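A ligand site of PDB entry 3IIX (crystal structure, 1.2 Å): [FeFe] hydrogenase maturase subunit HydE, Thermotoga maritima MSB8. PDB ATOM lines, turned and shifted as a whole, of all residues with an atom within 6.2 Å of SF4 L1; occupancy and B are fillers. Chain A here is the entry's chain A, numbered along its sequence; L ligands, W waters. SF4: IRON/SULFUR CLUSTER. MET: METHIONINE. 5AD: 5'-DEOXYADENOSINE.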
ATOM      1  N   VAL A  62      18.816  19.260   6.078  1.00  0.00           N
ATOM      2  CA  VAL A  62      17.503  18.893   6.647  1.00  0.00           C
ATOM      3  C   VAL A  62      16.390  19.572   5.851  1.00  0.00           C
ATOM      4  O   VAL A  62      16.478  20.752   5.539  1.00  0.00           O
ATOM      5  CB  VAL A  62      17.422  19.294   8.114  1.00  0.00           C
ATOM      6  CG1 VAL A  62      15.981  19.103   8.696  1.00  0.00           C
ATOM      7  CG2 VAL A  62      18.448  18.548   8.938  1.00  0.00           C
ATOM      8  N   CYS A  63      15.379  18.814   5.477  1.00  0.00           N
ATOM      9  CA  CYS A  63      14.250  19.397   4.765  1.00  0.00           C
ATOM     10  C   CYS A  63      12.925  18.808   5.202  1.00  0.00           C
ATOM     11  O   CYS A  63      12.785  17.589   5.355  1.00  0.00           O
ATOM     12  CB  CYS A  63      14.403  19.259   3.237  1.00  0.00           C
ATOM     13  SG  CYS A  63      13.232  20.412   2.398  1.00  0.00           S
ATOM     14  N   ARG A  64      11.954  19.690   5.356  1.00  0.00           N
ATOM     15  CA  ARG A  64      10.568  19.296   5.665  1.00  0.00           C
ATOM     16  C   ARG A  64       9.730  18.960   4.433  1.00  0.00           C
ATOM     17  O   ARG A  64       8.633  18.423   4.588  1.00  0.00           O
ATOM     18  CB  ARG A  64       9.853  20.416   6.399  1.00  0.00           C
ATOM     19  CG  ARG A  64       9.620  21.679   5.539  1.00  0.00           C
ATOM     20  CD  ARG A  64       9.063  22.802   6.325  1.00  0.00           C
ATOM     21  NE  ARG A  64       8.931  24.015   5.534  1.00  0.00           N
ATOM     22  CZ  ARG A  64       8.225  25.080   5.859  1.00  0.00           C
ATOM     23  NH1 ARG A  64       7.599  25.167   7.027  1.00  0.00           N
ATOM     24  NH2 ARG A  64       8.204  26.122   5.047  1.00  0.00           N
ATOM     25  N   LYS A  65      10.185  19.330   3.237  1.00  0.00           N
ATOM     26  CA  LYS A  65       9.442  19.095   2.002  1.00  0.00           C
ATOM     27  C   LYS A  65       9.895  17.802   1.350  1.00  0.00           C
ATOM     28  O   LYS A  65      10.879  17.196   1.741  1.00  0.00           O
ATOM     29  CB  LYS A  65       9.559  20.258   1.027  1.00  0.00           C
ATOM     30  CG  LYS A  65       8.625  21.399   1.352  1.00  0.00           C
ATOM     31  CD  LYS A  65       8.684  22.513   0.300  1.00  0.00           C
ATOM     32  CE  LYS A  65       7.559  23.571   0.448  1.00  0.00           C
ATOM     33  NZ  LYS A  65       7.370  24.134   1.800  1.00  0.00           N
ATOM     34  N   ASN A  66       9.138  17.377   0.343  1.00  0.00           N
ATOM     35  CA  ASN A  66       9.248  16.039  -0.245  1.00  0.00           C
ATOM     36  C   ASN A  66       9.309  16.076  -1.768  1.00  0.00           C
ATOM     37  O   ASN A  66       8.808  15.181  -2.440  1.00  0.00           O
ATOM     38  CB  ASN A  66       8.113  15.145   0.267  1.00  0.00           C
ATOM     39  CG  ASN A  66       8.494  13.672   0.363  1.00  0.00           C
ATOM     40  OD1 ASN A  66       9.644  13.322   0.526  1.00  0.00           O
ATOM     41  ND2 ASN A  66       7.484  12.804   0.327  1.00  0.00           N
ATOM     42  N   CYS A  67       9.909  17.116  -2.331  1.00  0.00           N
ATOM     43  CA  CYS A  67       9.956  17.278  -3.797  1.00  0.00           C
ATOM     44  C   CYS A  67      10.475  15.996  -4.438  1.00  0.00           C
ATOM     45  O   CYS A  67      11.457  15.410  -3.980  1.00  0.00           O
ATOM     46  CB  CYS A  67      10.887  18.460  -4.135  1.00  0.00           C
ATOM     47  SG  CYS A  67      10.409  20.014  -3.323  1.00  0.00           S
ATOM     48  N   TYR A  69      12.024  15.198  -7.105  1.00  0.00           N
ATOM     49  CA  TYR A  69      13.309  15.178  -7.841  1.00  0.00           C
ATOM     50  C   TYR A  69      14.525  15.263  -6.928  1.00  0.00           C
ATOM     51  O   TYR A  69      15.631  14.967  -7.372  1.00  0.00           O
ATOM     52  CB  TYR A  69      13.386  16.379  -8.806  1.00  0.00           C
ATOM     53  CG  TYR A  69      12.877  17.692  -8.271  1.00  0.00           C
ATOM     54  CD1 TYR A  69      13.681  18.485  -7.456  1.00  0.00           C
ATOM     55  CD2 TYR A  69      11.587  18.140  -8.544  1.00  0.00           C
ATOM     56  CE1 TYR A  69      13.229  19.692  -6.960  1.00  0.00           C
ATOM     57  CE2 TYR A  69      11.134  19.346  -8.049  1.00  0.00           C
ATOM     58  CZ  TYR A  69      11.969  20.111  -7.242  1.00  0.00           C
ATOM     59  OH  TYR A  69      11.461  21.295  -6.761  1.00  0.00           O
ATOM     60  N   CYS A  70      14.333  15.620  -5.667  1.00  0.00           N
ATOM     61  CA  CYS A  70      15.428  16.130  -4.813  1.00  0.00           C
ATOM     62  C   CYS A  70      15.972  15.073  -3.870  1.00  0.00           C
ATOM     63  O   CYS A  70      15.221  14.481  -3.103  1.00  0.00           O
ATOM     64  CB  CYS A  70      14.987  17.355  -3.998  1.00  0.00           C
ATOM     65  SG  CYS A  70      16.292  18.065  -3.043  1.00  0.00           S
ATOM     66  N   GLY A  71      17.292  14.885  -3.867  1.00  0.00           N
ATOM     67  CA  GLY A  71      17.910  13.986  -2.947  1.00  0.00           C
ATOM     68  C   GLY A  71      17.802  14.334  -1.473  1.00  0.00           C
ATOM     69  O   GLY A  71      18.125  13.481  -0.650  1.00  0.00           O
ATOM     70  N   LEU A  72      17.390  15.552  -1.114  1.00  0.00           N
ATOM     71  CA  LEU A  72      17.208  15.936   0.295  1.00  0.00           C
ATOM     72  C   LEU A  72      15.775  15.749   0.757  1.00  0.00           C
ATOM     73  O   LEU A  72      15.456  16.085   1.888  1.00  0.00           O
ATOM     74  CB  LEU A  72      17.640  17.397   0.592  1.00  0.00           C
ATOM     75  CG  LEU A  72      19.005  17.787   0.021  1.00  0.00           C
ATOM     76  CD1 LEU A  72      19.342  19.204   0.510  1.00  0.00           C
ATOM     77  CD2 LEU A  72      20.104  16.794   0.328  1.00  0.00           C
ATOM     78  N   ARG A  73      14.906  15.251  -0.117  1.00  0.00           N
ATOM     79  CA  ARG A  73      13.472  15.128   0.234  1.00  0.00           C
ATOM     80  C   ARG A  73      13.300  14.378   1.556  1.00  0.00           C
ATOM     81  O   ARG A  73      14.050  13.469   1.863  1.00  0.00           O
ATOM     82  CB  ARG A  73      12.702  14.465  -0.889  1.00  0.00           C
ATOM     83  CG  ARG A  73      13.085  13.009  -1.147  1.00  0.00           C
ATOM     84  CD  ARG A  73      12.617  12.518  -2.520  1.00  0.00           C
ATOM     85  NE  ARG A  73      11.196  12.783  -2.708  1.00  0.00           N
ATOM     86  CZ  ARG A  73      10.225  11.938  -2.383  1.00  0.00           C
ATOM     87  NH1 ARG A  73      10.501  10.740  -1.862  1.00  0.00           N
ATOM     88  NH2 ARG A  73       8.968  12.295  -2.584  1.00  0.00           N
ATOM     89  N   ARG A  74      12.267  14.751   2.311  1.00  0.00           N
ATOM     90  CA  ARG A  74      12.157  14.238   3.685  1.00  0.00           C
ATOM     91  C   ARG A  74      12.035  12.721   3.747  1.00  0.00           C
ATOM     92  O   ARG A  74      12.482  12.116   4.694  1.00  0.00           O
ATOM     93  CB  ARG A  74      11.056  14.886   4.505  1.00  0.00           C
ATOM     94  CG  ARG A  74       9.687  14.651   4.004  1.00  0.00           C
ATOM     95  CD  ARG A  74       8.599  15.060   5.034  1.00  0.00           C
ATOM     96  NE  ARG A  74       7.358  14.594   4.462  1.00  0.00           N
ATOM     97  CZ  ARG A  74       6.587  15.299   3.648  1.00  0.00           C
ATOM     98  NH1 ARG A  74       6.825  16.573   3.380  1.00  0.00           N
ATOM     99  NH2 ARG A  74       5.551  14.732   3.084  1.00  0.00           N
ATOM    100  N   SER A 108      20.012  25.970   1.974  1.00  0.00           N
ATOM    101  CA  SER A 108      19.712  24.830   2.793  1.00  0.00           C
ATOM    102  C   SER A 108      18.453  24.139   2.279  1.00  0.00           C
ATOM    103  O   SER A 108      17.666  24.695   1.490  1.00  0.00           O
ATOM    104  CB  SER A 108      19.530  25.234   4.240  1.00  0.00           C
ATOM    105  OG  SER A 108      18.436  26.124   4.395  1.00  0.00           O
ATOM    106  N   GLY A 109      18.223  22.925   2.794  1.00  0.00           N
ATOM    107  CA  GLY A 109      16.849  22.413   2.775  1.00  0.00           C
ATOM    108  C   GLY A 109      15.965  23.329   3.595  1.00  0.00           C
ATOM    109  O   GLY A 109      16.441  24.206   4.312  1.00  0.00           O
ATOM    110  N   GLU A 110      14.662  23.124   3.498  1.00  0.00           N
ATOM    111  CA  GLU A 110      13.730  23.875   4.353  1.00  0.00           C
ATOM    112  C   GLU A 110      13.781  23.293   5.753  1.00  0.00           C
ATOM    113  O   GLU A 110      12.957  22.446   6.149  1.00  0.00           O
ATOM    114  CB  GLU A 110      12.306  23.852   3.794  1.00  0.00           C
ATOM    115  CG  GLU A 110      12.162  24.613   2.483  1.00  0.00           C
ATOM    116  CD  GLU A 110      10.720  24.905   2.130  1.00  0.00           C
ATOM    117  OE1 GLU A 110       9.825  24.586   2.951  1.00  0.00           O
ATOM    118  OE2 GLU A 110      10.447  25.446   1.030  1.00  0.00           O
ATOM    119  N   GLY A 138      14.133  28.448   0.520  1.00  0.00           N
ATOM    120  CA  GLY A 138      12.836  27.888   0.198  1.00  0.00           C
ATOM    121  C   GLY A 138      11.691  28.839   0.559  1.00  0.00           C
ATOM    122  O   GLY A 138      11.852  30.070   0.645  1.00  0.00           O
ATOM    123  N   GLU A 161      11.019  26.495 -10.750  1.00  0.00           N
ATOM    124  CA  GLU A 161      11.105  25.037 -10.996  1.00  0.00           C
ATOM    125  C   GLU A 161      10.427  24.607 -12.292  1.00  0.00           C
ATOM    126  O   GLU A 161      11.058  24.039 -13.170  1.00  0.00           O
ATOM    127  CB  GLU A 161      10.602  24.213  -9.810  1.00  0.00           C
ATOM    128  CG  GLU A 161      11.213  24.575  -8.454  1.00  0.00           C
ATOM    129  CD  GLU A 161      12.709  24.457  -8.349  1.00  0.00           C
ATOM    130  OE1 GLU A 161      13.410  24.176  -9.344  1.00  0.00           O
ATOM    131  OE2 GLU A 161      13.207  24.697  -7.219  1.00  0.00           O
ATOM    132  N   ARG A 172       6.022  18.714  -6.513  1.00  0.00           N
ATOM    133  CA  ARG A 172       6.275  19.438  -5.275  1.00  0.00           C
ATOM    134  C   ARG A 172       4.991  19.359  -4.448  1.00  0.00           C
ATOM    135  O   ARG A 172       4.229  20.345  -4.326  1.00  0.00           O
ATOM    136  CB  ARG A 172       6.698  20.859  -5.595  1.00  0.00           C
ATOM    137  CG  ARG A 172       7.845  20.915  -6.611  1.00  0.00           C
ATOM    138  CD  ARG A 172       8.485  22.295  -6.706  1.00  0.00           C
ATOM    139  NE  ARG A 172       9.165  22.624  -5.449  1.00  0.00           N
ATOM    140  CZ  ARG A 172       8.807  23.557  -4.591  1.00  0.00           C
ATOM    141  NH1 ARG A 172       7.825  24.411  -4.863  1.00  0.00           N
ATOM    142  NH2 ARG A 172       9.442  23.639  -3.432  1.00  0.00           N
ATOM    143  N   ARG A 180       4.566  29.345  -4.958  1.00  0.00           N
ATOM    144  CA  ARG A 180       5.918  29.694  -5.371  1.00  0.00           C
ATOM    145  C   ARG A 180       5.957  31.084  -5.984  1.00  0.00           C
ATOM    146  O   ARG A 180       6.825  31.886  -5.666  1.00  0.00           O
ATOM    147  CB  ARG A 180       6.408  28.664  -6.383  1.00  0.00           C
ATOM    148  CG  ARG A 180       7.909  28.603  -6.587  1.00  0.00           C
ATOM    149  CD  ARG A 180       8.592  27.958  -5.384  1.00  0.00           C
ATOM    150  NE  ARG A 180       9.976  27.615  -5.645  1.00  0.00           N
ATOM    151  CZ  ARG A 180      10.805  27.074  -4.762  1.00  0.00           C
ATOM    152  NH1 ARG A 180      10.379  26.768  -3.542  1.00  0.00           N
ATOM    153  NH2 ARG A 180      12.059  26.817  -5.107  1.00  0.00           N
ATOM    154  N   TYR A 303      25.363  16.816   0.750  1.00  0.00           N
ATOM    155  CA  TYR A 303      24.391  17.742   0.140  1.00  0.00           C
ATOM    156  C   TYR A 303      24.383  17.495  -1.343  1.00  0.00           C
ATOM    157  O   TYR A 303      25.037  18.183  -2.111  1.00  0.00           O
ATOM    158  CB  TYR A 303      24.768  19.166   0.438  1.00  0.00           C
ATOM    159  CG  TYR A 303      23.703  20.200   0.182  1.00  0.00           C
ATOM    160  CD1 TYR A 303      22.882  20.647   1.216  1.00  0.00           C
ATOM    161  CD2 TYR A 303      23.563  20.789  -1.064  1.00  0.00           C
ATOM    162  CE1 TYR A 303      21.973  21.660   1.051  1.00  0.00           C
ATOM    163  CE2 TYR A 303      22.628  21.809  -1.241  1.00  0.00           C
ATOM    164  CZ  TYR A 303      21.860  22.242  -0.183  1.00  0.00           C
ATOM    165  OH  TYR A 303      20.986  23.284  -0.359  1.00  0.00           O
ATOM    166  N   LEU A 305      21.735  17.102  -4.112  1.00  0.00           N
ATOM    167  CA  LEU A 305      20.387  17.219  -4.631  1.00  0.00           C
ATOM    168  C   LEU A 305      20.208  16.240  -5.777  1.00  0.00           C
ATOM    169  O   LEU A 305      19.139  15.669  -5.962  1.00  0.00           O
ATOM    170  CB  LEU A 305      20.134  18.651  -5.117  1.00  0.00           C
ATOM    171  CG  LEU A 305      20.555  19.794  -4.192  1.00  0.00           C
ATOM    172  CD1 LEU A 305      20.053  21.128  -4.732  1.00  0.00           C
ATOM    173  CD2 LEU A 305      20.070  19.552  -2.800  1.00  0.00           C
HETATM  174 FE1  SF4 L   1      12.410  20.544  -2.268  1.00  0.00          FE
HETATM  175 FE2  SF4 L   1      14.598  22.476  -1.773  1.00  0.00          FE
HETATM  176 FE3  SF4 L   1      13.631  20.446   0.158  1.00  0.00          FE
HETATM  177 FE4  SF4 L   1      14.961  19.626  -2.025  1.00  0.00          FE
HETATM  178  S1  SF4 L   1      15.796  20.933  -0.386  1.00  0.00           S
HETATM  179  S2  SF4 L   1      13.074  18.646  -1.105  1.00  0.00           S
HETATM  180  S3  SF4 L   1      14.190  21.098  -3.634  1.00  0.00           S
HETATM  181  S4  SF4 L   1      12.416  22.208  -0.702  1.00  0.00           S
HETATM  182  N   MET L   2      15.125  24.223  -0.474  1.00  0.00           N
HETATM  183  CA  MET L   2      15.314  25.495  -1.217  1.00  0.00           C
HETATM  184  C   MET L   2      14.444  25.444  -2.462  1.00  0.00           C
HETATM  185  O   MET L   2      14.220  26.505  -3.108  1.00  0.00           O
HETATM  186  CB  MET L   2      16.774  25.636  -1.642  1.00  0.00           C
HETATM  187  CG  MET L   2      17.150  24.923  -2.920  1.00  0.00           C
HETATM  188  SD  MET L   2      16.939  23.129  -2.874  1.00  0.00           S
HETATM  189  CE  MET L   2      18.258  22.769  -1.692  1.00  0.00           C
HETATM  190  OXT MET L   2      13.946  24.359  -2.846  1.00  0.00           O
HETATM  191  N1  5AD L   3      18.458  17.657 -10.709  1.00  0.00           N
HETATM  192  C2  5AD L   3      18.801  18.934 -11.110  1.00  0.00           C
HETATM  193  N3  5AD L   3      18.540  20.015 -10.333  1.00  0.00           N
HETATM  194  C4  5AD L   3      17.958  19.813  -9.131  1.00  0.00           C
HETATM  195  N9  5AD L   3      17.575  20.705  -8.188  1.00  0.00           N
HETATM  196  C8  5AD L   3      17.042  20.004  -7.138  1.00  0.00           C
HETATM  197  N7  5AD L   3      17.078  18.684  -7.420  1.00  0.00           N
HETATM  198  C5  5AD L   3      17.621  18.525  -8.673  1.00  0.00           C
HETATM  199  C6  5AD L   3      17.906  17.447  -9.478  1.00  0.00           C
HETATM  200  N6  5AD L   3      17.611  16.183  -9.127  1.00  0.00           N
HETATM  201  C1' 5AD L   3      17.652  22.166  -8.359  1.00  0.00           C
HETATM  202  C2' 5AD L   3      16.284  22.835  -8.146  1.00  0.00           C
HETATM  203  C3' 5AD L   3      16.529  23.745  -6.961  1.00  0.00           C
HETATM  204  C4' 5AD L   3      18.013  24.037  -7.145  1.00  0.00           C
HETATM  205  C5' 5AD L   3      18.763  24.510  -5.912  1.00  0.00           C
HETATM  206  O4' 5AD L   3      18.558  22.764  -7.482  1.00  0.00           O
HETATM  207  O2' 5AD L   3      15.968  23.543  -9.328  1.00  0.00           O
HETATM  208  O3' 5AD L   3      15.777  24.946  -6.961  1.00  0.00           O
HETATM  209  O   HOH W   1      11.363  25.229  -1.462  1.00  0.00           O
HETATM  210  O   HOH W   2      12.204  23.285  -5.068  1.00  0.00           O
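CB of Lys 65 touches S4 of SF4 L1 (3.9 Å).
Tyr 69 touches SF4 L1.
Arg 73 touches SF4 L1 (CA to S2, 3.8 Å).
Gly 109 touches SF4 L1 (CA to S1, 3.6 Å).
Glu 110 touches SF4 L1.
Hydrophobic or aromatic side chains within 4 Å of SF4 L1: Tyr 69.
The nearest printed residue that does not touch SF4 L1 is Leu 72 (4.05 Å).
The guanidinium group of Arg 73 lies within hydrogen-bond range of the backbone carbonyl oxygen of Cys 67.
The side-chain sulfur of Cys 63 lies close to the backbone NH of Lys 65 (3.3 Å).
The guanidinium group (NH2) of Arg 73 lies within hydrogen-bond range of the backbone carbonyl oxygen (O) of Asn 66, 2.9 Å away.
SG of Cys 67 sits close to NE of Arg 172, at 3.6 Å.
N of Leu 72 lies close to SG of Cys 70, at 3.4 Å.
O of Lys 65 is in hydrogen-bond range of N of Arg 74 (2.9 Å).
N of Glu 110 lies close to SG of Cys 63.
NZ of Lys 65 lies within salt-bridge range of OE1 of Glu 110, at 2.7 Å.
An iron atom (FE3) of SF4 L1 is bound by the side-chain sulfur (SG) of Cys 63.
O of Tyr 69 is in hydrogen-bond range of N6 of 5AD L3, at 2.9 Å.
FE1 of SF4 L1 is bound by SG of Cys 67, 2.3 Å away.
The backbone carbonyl oxygen (O) of Ser 108 lies close to a nitrogen (N) of MET L2 (3.2 Å).
The backbone NH (N) of Cys 67 sits close to a sulfur (S2) of SF4 L1 (3.7 Å).
An oxygen (O3') of 5AD L3 lies within hydrogen-bond range of the side-chain carboxylate (OE2) of Glu 161.
The guanidinium group (NH2) of Arg 180 is in salt-bridge range of an oxygen (O) of MET L2 (3.0 Å).
SG of Cys 70 is bound to FE4 of SF4 L1 (2.3 Å).
A nitrogen (N) of MET L2 is bound to an iron atom (FE2) of SF4 L1, 2.2 Å away.
Water W2 lies within hydrogen-bond range of the side-chain hydroxyl of Tyr 69, the side-chain carboxylate of Glu 161, the guanidinium group of Arg 172 and a sulfur (S3) of SF4 L1.
Water W1 lies within hydrogen-bond range of OE2 of Glu 110 (2.7 Å), NH1 of Arg 180 (2.8 Å), NH2 of Arg 172 (3.2 Å) and S4 of SF4 L1 (3.3 Å).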
